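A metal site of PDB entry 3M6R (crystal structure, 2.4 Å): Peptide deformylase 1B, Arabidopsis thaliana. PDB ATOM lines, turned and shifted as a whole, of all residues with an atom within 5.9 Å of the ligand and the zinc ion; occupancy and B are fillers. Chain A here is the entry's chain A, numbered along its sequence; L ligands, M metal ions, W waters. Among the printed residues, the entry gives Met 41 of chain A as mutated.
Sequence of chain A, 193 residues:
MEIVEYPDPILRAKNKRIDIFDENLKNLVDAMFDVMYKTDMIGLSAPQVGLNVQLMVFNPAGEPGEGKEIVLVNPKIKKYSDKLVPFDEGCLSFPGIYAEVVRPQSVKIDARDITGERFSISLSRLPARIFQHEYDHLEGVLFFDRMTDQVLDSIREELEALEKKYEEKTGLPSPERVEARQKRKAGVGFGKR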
ATOM      1  N   THR A  39     -32.918  -3.457  20.045  1.00  0.00           N
ATOM      2  CA  THR A  39     -32.819  -3.958  18.681  1.00  0.00           C
ATOM      3  C   THR A  39     -32.623  -5.463  18.627  1.00  0.00           C
ATOM      4  O   THR A  39     -32.401  -6.018  17.552  1.00  0.00           O
ATOM      5  CB  THR A  39     -31.665  -3.268  17.903  1.00  0.00           C
ATOM      6  OG1 THR A  39     -30.420  -3.519  18.559  1.00  0.00           O
ATOM      7  CG2 THR A  39     -31.899  -1.755  17.831  1.00  0.00           C
ATOM      8  N   ASP A  40     -32.711  -6.107  19.783  1.00  0.00           N
ATOM      9  CA  ASP A  40     -32.537  -7.562  19.883  1.00  0.00           C
ATOM     10  C   ASP A  40     -31.181  -8.072  19.410  1.00  0.00           C
ATOM     11  O   ASP A  40     -31.098  -9.139  18.800  1.00  0.00           O
ATOM     12  CB  ASP A  40     -33.645  -8.284  19.114  1.00  0.00           C
ATOM     13  CG  ASP A  40     -34.767  -8.747  20.009  1.00  0.00           C
ATOM     14  OD1 ASP A  40     -35.510  -7.887  20.544  1.00  0.00           O
ATOM     15  OD2 ASP A  40     -34.901  -9.974  20.196  1.00  0.00           O
ATOM     16  N   MET A  41     -30.122  -7.319  19.662  1.00  0.00           N
ATOM     17  CA  MET A  41     -28.790  -7.745  19.263  1.00  0.00           C
ATOM     18  C   MET A  41     -28.076  -8.334  20.491  1.00  0.00           C
ATOM     19  O   MET A  41     -28.601  -8.285  21.595  1.00  0.00           O
ATOM     20  CB  MET A  41     -27.999  -6.561  18.692  1.00  0.00           C
ATOM     21  CG  MET A  41     -28.592  -5.938  17.416  1.00  0.00           C
ATOM     22  SD  MET A  41     -28.988  -7.099  16.069  1.00  0.00           S
ATOM     23  CE  MET A  41     -27.935  -6.682  14.904  1.00  0.00           C
ATOM     24  N   ILE A  42     -26.902  -8.919  20.288  1.00  0.00           N
ATOM     25  CA  ILE A  42     -26.175  -9.472  21.430  1.00  0.00           C
ATOM     26  C   ILE A  42     -24.887  -8.714  21.653  1.00  0.00           C
ATOM     27  O   ILE A  42     -24.108  -9.048  22.553  1.00  0.00           O
ATOM     28  CB  ILE A  42     -25.855 -10.970  21.270  1.00  0.00           C
ATOM     29  CG1 ILE A  42     -25.085 -11.224  19.978  1.00  0.00           C
ATOM     30  CG2 ILE A  42     -27.150 -11.777  21.304  1.00  0.00           C
ATOM     31  CD1 ILE A  42     -24.762 -12.679  19.739  1.00  0.00           C
ATOM     32  N   GLY A  43     -24.676  -7.683  20.830  1.00  0.00           N
ATOM     33  CA  GLY A  43     -23.480  -6.862  20.937  1.00  0.00           C
ATOM     34  C   GLY A  43     -23.638  -5.557  20.177  1.00  0.00           C
ATOM     35  O   GLY A  43     -24.588  -5.400  19.410  1.00  0.00           O
ATOM     36  N   LEU A  44     -22.705  -4.639  20.371  1.00  0.00           N
ATOM     37  CA  LEU A  44     -22.778  -3.347  19.697  1.00  0.00           C
ATOM     38  C   LEU A  44     -21.453  -2.590  19.773  1.00  0.00           C
ATOM     39  O   LEU A  44     -20.740  -2.662  20.782  1.00  0.00           O
ATOM     40  CB  LEU A  44     -23.904  -2.516  20.320  1.00  0.00           C
ATOM     41  CG  LEU A  44     -24.399  -1.292  19.565  1.00  0.00           C
ATOM     42  CD1 LEU A  44     -24.896  -1.689  18.184  1.00  0.00           C
ATOM     43  CD2 LEU A  44     -25.510  -0.640  20.376  1.00  0.00           C
ATOM     44  N   SER A  45     -21.109  -1.884  18.712  1.00  0.00           N
ATOM     45  CA  SER A  45     -19.872  -1.101  18.700  1.00  0.00           C
ATOM     46  C   SER A  45     -20.241   0.373  18.539  1.00  0.00           C
ATOM     47  O   SER A  45     -21.329   0.698  18.075  1.00  0.00           O
ATOM     48  CB  SER A  45     -18.930  -1.545  17.574  1.00  0.00           C
ATOM     49  OG  SER A  45     -19.477  -1.262  16.290  1.00  0.00           O
ATOM     50  N   GLN A  48     -21.571   2.139  15.158  1.00  0.00           N
ATOM     51  CA  GLN A  48     -22.945   1.833  14.820  1.00  0.00           C
ATOM     52  C   GLN A  48     -23.971   2.802  15.383  1.00  0.00           C
ATOM     53  O   GLN A  48     -25.141   2.805  14.972  1.00  0.00           O
ATOM     54  CB  GLN A  48     -23.254   0.401  15.247  1.00  0.00           C
ATOM     55  CG  GLN A  48     -22.449  -0.616  14.472  1.00  0.00           C
ATOM     56  CD  GLN A  48     -22.668  -2.031  14.948  1.00  0.00           C
ATOM     57  OE1 GLN A  48     -22.125  -2.432  15.969  1.00  0.00           O
ATOM     58  NE2 GLN A  48     -23.490  -2.781  14.213  1.00  0.00           N
ATOM     59  N   PHE A  87     -19.825 -19.991  11.412  1.00  0.00           N
ATOM     60  CA  PHE A  87     -20.961 -19.601  12.239  1.00  0.00           C
ATOM     61  C   PHE A  87     -21.763 -18.522  11.505  1.00  0.00           C
ATOM     62  O   PHE A  87     -21.194 -17.639  10.866  1.00  0.00           O
ATOM     63  CB  PHE A  87     -20.449 -19.110  13.597  1.00  0.00           C
ATOM     64  CG  PHE A  87     -21.512 -19.026  14.648  1.00  0.00           C
ATOM     65  CD1 PHE A  87     -22.055 -17.799  15.005  1.00  0.00           C
ATOM     66  CD2 PHE A  87     -21.987 -20.173  15.269  1.00  0.00           C
ATOM     67  CE1 PHE A  87     -23.071 -17.721  15.974  1.00  0.00           C
ATOM     68  CE2 PHE A  87     -22.996 -20.110  16.232  1.00  0.00           C
ATOM     69  CZ  PHE A  87     -23.540 -18.871  16.576  1.00  0.00           C
ATOM     70  N   ASP A  88     -23.088 -18.593  11.568  1.00  0.00           N
ATOM     71  CA  ASP A  88     -23.918 -17.612  10.895  1.00  0.00           C
ATOM     72  C   ASP A  88     -23.983 -16.320  11.692  1.00  0.00           C
ATOM     73  O   ASP A  88     -24.117 -16.335  12.922  1.00  0.00           O
ATOM     74  CB  ASP A  88     -25.336 -18.144  10.656  1.00  0.00           C
ATOM     75  CG  ASP A  88     -25.375 -19.230   9.592  1.00  0.00           C
ATOM     76  OD1 ASP A  88     -24.722 -19.063   8.547  1.00  0.00           O
ATOM     77  OD2 ASP A  88     -26.091 -20.245   9.800  1.00  0.00           O
ATOM     78  N   GLU A  89     -23.889 -15.196  10.981  1.00  0.00           N
ATOM     79  CA  GLU A  89     -23.888 -13.888  11.614  1.00  0.00           C
ATOM     80  C   GLU A  89     -24.853 -12.896  11.000  1.00  0.00           C
ATOM     81  O   GLU A  89     -25.118 -12.915   9.793  1.00  0.00           O
ATOM     82  CB  GLU A  89     -22.499 -13.263  11.561  1.00  0.00           C
ATOM     83  CG  GLU A  89     -21.464 -13.803  12.525  1.00  0.00           C
ATOM     84  CD  GLU A  89     -20.101 -13.166  12.317  1.00  0.00           C
ATOM     85  OE1 GLU A  89     -20.044 -11.930  12.090  1.00  0.00           O
ATOM     86  OE2 GLU A  89     -19.075 -13.879  12.370  1.00  0.00           O
ATOM     87  N   GLY A  90     -25.359 -12.006  11.848  1.00  0.00           N
ATOM     88  CA  GLY A  90     -26.221 -10.933  11.392  1.00  0.00           C
ATOM     89  C   GLY A  90     -25.485  -9.653  11.792  1.00  0.00           C
ATOM     90  O   GLY A  90     -24.444  -9.738  12.445  1.00  0.00           O
ATOM     91  N   CYS A  91     -25.976  -8.482  11.400  1.00  0.00           N
ATOM     92  CA  CYS A  91     -25.364  -7.199  11.780  1.00  0.00           C
ATOM     93  C   CYS A  91     -26.410  -6.081  11.730  1.00  0.00           C
ATOM     94  O   CYS A  91     -27.116  -5.896  10.715  1.00  0.00           O
ATOM     95  CB  CYS A  91     -24.177  -6.867  10.860  1.00  0.00           C
ATOM     96  SG  CYS A  91     -23.217  -5.324  11.261  1.00  0.00           S
ATOM     97  N   LEU A  92     -26.523  -5.346  12.824  1.00  0.00           N
ATOM     98  CA  LEU A  92     -27.462  -4.239  12.937  1.00  0.00           C
ATOM     99  C   LEU A  92     -27.250  -3.180  11.839  1.00  0.00           C
ATOM    100  O   LEU A  92     -28.163  -2.422  11.525  1.00  0.00           O
ATOM    101  CB  LEU A  92     -27.322  -3.589  14.315  1.00  0.00           C
ATOM    102  CG  LEU A  92     -28.192  -2.391  14.701  1.00  0.00           C
ATOM    103  CD1 LEU A  92     -29.672  -2.799  14.823  1.00  0.00           C
ATOM    104  CD2 LEU A  92     -27.689  -1.848  16.028  1.00  0.00           C
ATOM    105  N   SER A  93     -26.069  -3.127  11.243  1.00  0.00           N
ATOM    106  CA  SER A  93     -25.825  -2.143  10.206  1.00  0.00           C
ATOM    107  C   SER A  93     -26.251  -2.616   8.803  1.00  0.00           C
ATOM    108  O   SER A  93     -26.253  -1.846   7.845  1.00  0.00           O
ATOM    109  CB  SER A  93     -24.357  -1.714  10.224  1.00  0.00           C
ATOM    110  OG  SER A  93     -24.002  -1.156  11.481  1.00  0.00           O
ATOM    111  N   TYR A  98     -28.108 -12.239   6.579  1.00  0.00           N
ATOM    112  CA  TYR A  98     -27.496 -13.287   7.397  1.00  0.00           C
ATOM    113  C   TYR A  98     -26.615 -14.165   6.524  1.00  0.00           C
ATOM    114  O   TYR A  98     -26.991 -14.545   5.421  1.00  0.00           O
ATOM    115  CB  TYR A  98     -28.544 -14.180   8.046  1.00  0.00           C
ATOM    116  CG  TYR A  98     -29.498 -13.445   8.925  1.00  0.00           C
ATOM    117  CD1 TYR A  98     -29.460 -13.591  10.312  1.00  0.00           C
ATOM    118  CD2 TYR A  98     -30.474 -12.608   8.364  1.00  0.00           C
ATOM    119  CE1 TYR A  98     -30.379 -12.912  11.134  1.00  0.00           C
ATOM    120  CE2 TYR A  98     -31.399 -11.926   9.174  1.00  0.00           C
ATOM    121  CZ  TYR A  98     -31.340 -12.085  10.548  1.00  0.00           C
ATOM    122  OH  TYR A  98     -32.259 -11.407  11.329  1.00  0.00           O
ATOM    123  N   ARG A 103     -14.271 -17.673  11.392  1.00  0.00           N
ATOM    124  CA  ARG A 103     -13.416 -16.870  12.263  1.00  0.00           C
ATOM    125  C   ARG A 103     -12.657 -17.817  13.174  1.00  0.00           C
ATOM    126  O   ARG A 103     -13.033 -18.972  13.310  1.00  0.00           O
ATOM    127  CB  ARG A 103     -14.249 -15.916  13.157  1.00  0.00           C
ATOM    128  CG  ARG A 103     -14.975 -14.753  12.448  1.00  0.00           C
ATOM    129  CD  ARG A 103     -15.761 -13.916  13.466  1.00  0.00           C
ATOM    130  NE  ARG A 103     -16.674 -12.932  12.865  1.00  0.00           N
ATOM    131  CZ  ARG A 103     -16.316 -11.737  12.385  1.00  0.00           C
ATOM    132  NH1 ARG A 103     -17.241 -10.929  11.873  1.00  0.00           N
ATOM    133  NH2 ARG A 103     -15.055 -11.349  12.411  1.00  0.00           N
ATOM    134  N   LEU A 126     -19.067 -18.673  21.772  1.00  0.00           N
ATOM    135  CA  LEU A 126     -19.821 -17.511  21.359  1.00  0.00           C
ATOM    136  C   LEU A 126     -19.238 -16.142  21.759  1.00  0.00           C
ATOM    137  O   LEU A 126     -19.253 -15.187  20.977  1.00  0.00           O
ATOM    138  CB  LEU A 126     -21.261 -17.635  21.851  1.00  0.00           C
ATOM    139  CG  LEU A 126     -22.212 -16.520  21.408  1.00  0.00           C
ATOM    140  CD1 LEU A 126     -22.304 -16.507  19.883  1.00  0.00           C
ATOM    141  CD2 LEU A 126     -23.582 -16.740  22.026  1.00  0.00           C
ATOM    142  N   ARG A 129     -16.831 -15.066  19.422  1.00  0.00           N
ATOM    143  CA  ARG A 129     -17.461 -14.769  18.158  1.00  0.00           C
ATOM    144  C   ARG A 129     -17.932 -13.337  18.083  1.00  0.00           C
ATOM    145  O   ARG A 129     -17.703 -12.645  17.090  1.00  0.00           O
ATOM    146  CB  ARG A 129     -18.682 -15.646  17.960  1.00  0.00           C
ATOM    147  CG  ARG A 129     -19.190 -15.527  16.567  1.00  0.00           C
ATOM    148  CD  ARG A 129     -18.110 -16.092  15.713  1.00  0.00           C
ATOM    149  NE  ARG A 129     -18.352 -15.850  14.312  1.00  0.00           N
ATOM    150  CZ  ARG A 129     -17.893 -16.635  13.353  1.00  0.00           C
ATOM    151  NH1 ARG A 129     -17.175 -17.707  13.670  1.00  0.00           N
ATOM    152  NH2 ARG A 129     -18.179 -16.341  12.100  1.00  0.00           N
ATOM    153  N   ILE A 130     -18.635 -12.919  19.136  1.00  0.00           N
ATOM    154  CA  ILE A 130     -19.188 -11.586  19.276  1.00  0.00           C
ATOM    155  C   ILE A 130     -18.067 -10.549  19.330  1.00  0.00           C
ATOM    156  O   ILE A 130     -18.075  -9.574  18.598  1.00  0.00           O
ATOM    157  CB  ILE A 130     -20.036 -11.484  20.574  1.00  0.00           C
ATOM    158  CG1 ILE A 130     -21.122 -12.552  20.575  1.00  0.00           C
ATOM    159  CG2 ILE A 130     -20.652 -10.103  20.701  1.00  0.00           C
ATOM    160  CD1 ILE A 130     -21.934 -12.598  21.874  1.00  0.00           C
ATOM    161  N   HIS A 133     -16.469  -9.843  15.939  1.00  0.00           N
ATOM    162  CA  HIS A 133     -17.350  -9.126  15.035  1.00  0.00           C
ATOM    163  C   HIS A 133     -17.280  -7.621  15.372  1.00  0.00           C
ATOM    164  O   HIS A 133     -17.200  -6.770  14.483  1.00  0.00           O
ATOM    165  CB  HIS A 133     -18.784  -9.630  15.215  1.00  0.00           C
ATOM    166  CG  HIS A 133     -19.791  -8.943  14.348  1.00  0.00           C
ATOM    167  ND1 HIS A 133     -19.955  -9.255  13.014  1.00  0.00           N
ATOM    168  CD2 HIS A 133     -20.679  -7.968  14.620  1.00  0.00           C
ATOM    169  CE1 HIS A 133     -20.917  -8.506  12.513  1.00  0.00           C
ATOM    170  NE2 HIS A 133     -21.370  -7.714  13.462  1.00  0.00           N
ATOM    171  N   GLU A 134     -17.303  -7.317  16.672  1.00  0.00           N
ATOM    172  CA  GLU A 134     -17.249  -5.938  17.161  1.00  0.00           C
ATOM    173  C   GLU A 134     -15.855  -5.342  16.936  1.00  0.00           C
ATOM    174  O   GLU A 134     -15.709  -4.221  16.457  1.00  0.00           O
ATOM    175  CB  GLU A 134     -17.588  -5.908  18.646  1.00  0.00           C
ATOM    176  CG  GLU A 134     -18.830  -6.694  19.022  1.00  0.00           C
ATOM    177  CD  GLU A 134     -20.106  -6.146  18.394  1.00  0.00           C
ATOM    178  OE1 GLU A 134     -21.114  -6.891  18.362  1.00  0.00           O
ATOM    179  OE2 GLU A 134     -20.115  -4.980  17.953  1.00  0.00           O
ATOM    180  N   HIS A 137     -15.487  -4.183  13.723  1.00  0.00           N
ATOM    181  CA  HIS A 137     -16.167  -2.907  13.643  1.00  0.00           C
ATOM    182  C   HIS A 137     -15.268  -1.745  14.071  1.00  0.00           C
ATOM    183  O   HIS A 137     -15.193  -0.725  13.383  1.00  0.00           O
ATOM    184  CB  HIS A 137     -17.413  -2.904  14.527  1.00  0.00           C
ATOM    185  CG  HIS A 137     -18.678  -3.222  13.811  1.00  0.00           C
ATOM    186  ND1 HIS A 137     -19.200  -2.416  12.814  1.00  0.00           N
ATOM    187  CD2 HIS A 137     -19.562  -4.244  13.969  1.00  0.00           C
ATOM    188  CE1 HIS A 137     -20.350  -2.922  12.396  1.00  0.00           C
ATOM    189  NE2 HIS A 137     -20.587  -4.033  13.091  1.00  0.00           N
HETATM  190  C1  LIG L   1     -24.999  -7.036  16.365  1.00  0.00           C
HETATM  191  C2  LIG L   1     -23.690  -6.174  15.992  1.00  0.00           C
HETATM  192  O1  LIG L   1     -24.041  -5.793  14.866  1.00  0.00           O
HETATM  193  N1  LIG L   1     -22.526  -5.789  16.516  1.00  0.00           N
HETATM  194  O2  LIG L   1     -21.653  -4.992  15.788  1.00  0.00           O
HETATM  195  C3  LIG L   1     -24.628  -8.477  15.864  1.00  0.00           C
HETATM  196  C4  LIG L   1     -25.905  -9.288  16.267  1.00  0.00           C
HETATM  197  O3  LIG L   1     -26.335  -9.189  17.428  1.00  0.00           O
HETATM  198  C5  LIG L   1     -23.401  -9.016  16.657  1.00  0.00           C
HETATM  199  C6  LIG L   1     -23.072 -10.423  16.089  1.00  0.00           C
HETATM  200  C7  LIG L   1     -21.920 -11.094  16.770  1.00  0.00           C
HETATM  201  C8  LIG L   1     -21.591 -12.332  15.956  1.00  0.00           C
HETATM  202  C9  LIG L   1     -22.463 -13.505  16.391  1.00  0.00           C
HETATM  203  N2  LIG L   1     -26.379 -10.039  15.210  1.00  0.00           N
HETATM  204  C10 LIG L   1     -26.958 -11.288  15.791  1.00  0.00           C
HETATM  205  C11 LIG L   1     -28.463 -11.289  15.258  1.00  0.00           C
HETATM  206  C12 LIG L   1     -29.398 -10.402  16.126  1.00  0.00           C
HETATM  207  C13 LIG L   1     -28.570 -10.803  13.767  1.00  0.00           C
HETATM  208  C14 LIG L   1     -26.265 -12.605  15.297  1.00  0.00           C
HETATM  209  O4  LIG L   1     -25.385 -12.543  14.470  1.00  0.00           O
HETATM  210  N3  LIG L   1     -26.901 -13.757  16.141  1.00  0.00           N
HETATM  211  C15 LIG L   1     -26.426 -15.162  15.931  1.00  0.00           C
HETATM  212  C16 LIG L   1     -27.952 -13.818  17.228  1.00  0.00           C
HETATM  213  C17 LIG L   1     -27.551 -15.056  18.057  1.00  0.00           C
HETATM  214  C18 LIG L   1     -27.222 -16.045  16.921  1.00  0.00           C
HETATM  215  C19 LIG L   1     -26.717 -15.633  14.488  1.00  0.00           C
HETATM  216  O5  LIG L   1     -26.250 -16.963  14.285  1.00  0.00           O
HETATM  217 ZN    ZN M   1     -22.137  -5.647  13.390  1.00  0.00          ZN
HETATM  218  O   HOH W   1     -29.238 -18.059  18.421  1.00  0.00           O
HETATM  219  O   HOH W   2     -28.884 -17.310  12.052  1.00  0.00           O
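NE2 of His 133 binds the zinc ion (2.2 Å). NE2 of His 137 is bound to the zinc ion, at 2.3 Å. The side-chain sulfur (SG) of Cys 91 binds the zinc ion, at 2.4 Å. An oxygen (O1) of the ligand is bound to the zinc ion. O2 of the ligand binds the zinc ion.
An oxygen (O3) of the ligand lies close to the side-chain sulfur of Met 41, 3.6 Å away. Residues that only touch the ligand: Asp 40, Gly 43, Phe 87, Glu 89, Tyr 98, Arg 129 and Ile 130. Hydrophobic or aromatic side chains within 4 Å of the ligand: Met 41, Ile 42, Phe 87, Leu 92, Tyr 98, His 133 and His 137. Within 4 Å of the ligand: Asp 40, Met 41, Ile 42, Gly 43, Gln 48, Phe 87, Asp 88, Glu 89, Gly 90, Cys 91, Leu 92, Tyr 98, Arg 129, Ile 130, His 133, Glu 134 and His 137.
NE2 of Gln 48 touches the zinc ion, 3.3 Å away. Within 4 Å of the zinc ion: Gln 48, Cys 91, His 133 and His 137.
O1 of the ligand lies close to N of Leu 92, at 3.2 Å. The backbone NH (N) of Ile 42 sits at hydrogen-bond distance from an oxygen (O3) of the ligand. N1 of the ligand lies within hydrogen-bond range of OE1 of Gln 48. The backbone NH of Gly 90 is in hydrogen-bond range of an oxygen (O4) of the ligand (2.7 Å). A nitrogen (N1) of the ligand is in hydrogen-bond range of the side-chain carboxylate of Glu 134, at 2.6 Å. O of Asp 88 is in hydrogen-bond range of O5 of the ligand, at 2.6 Å. The backbone carbonyl oxygen of Gly 90 lies within hydrogen-bond range of a nitrogen (N2) of the ligand (3.4 Å).
A ring nitrogen (ND1) of His 133 lies within hydrogen-bond range of the side-chain carboxylate (OE1) of Glu 89 (2.8 Å). The side-chain hydroxyl (OG) of Ser 45 is in hydrogen-bond range of the side-chain amide oxygen (OE1) of Gln 48 (2.9 Å). OE2 of Glu 134 lies within hydrogen-bond range of N of Ser 45, at 3.3 Å. The side-chain hydroxyl (OG) of Ser 93 lies within hydrogen-bond range of the side-chain amide nitrogen (NE2) of Gln 48 (3.2 Å). The side-chain carboxylate of Glu 89 is in salt-bridge range of the guanidinium group of Arg 129 (2.6 Å). A ring nitrogen (NE2) of His 137 sits close to the side-chain amide nitrogen (NE2) of Gln 48 (3.4 Å). A ring nitrogen (ND1) of His 133 sits at hydrogen-bond distance from the guanidinium group (NH1) of Arg 103 (3.4 Å). OE1 of Glu 134 lies within hydrogen-bond range of N of Leu 44, at 3.4 Å.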
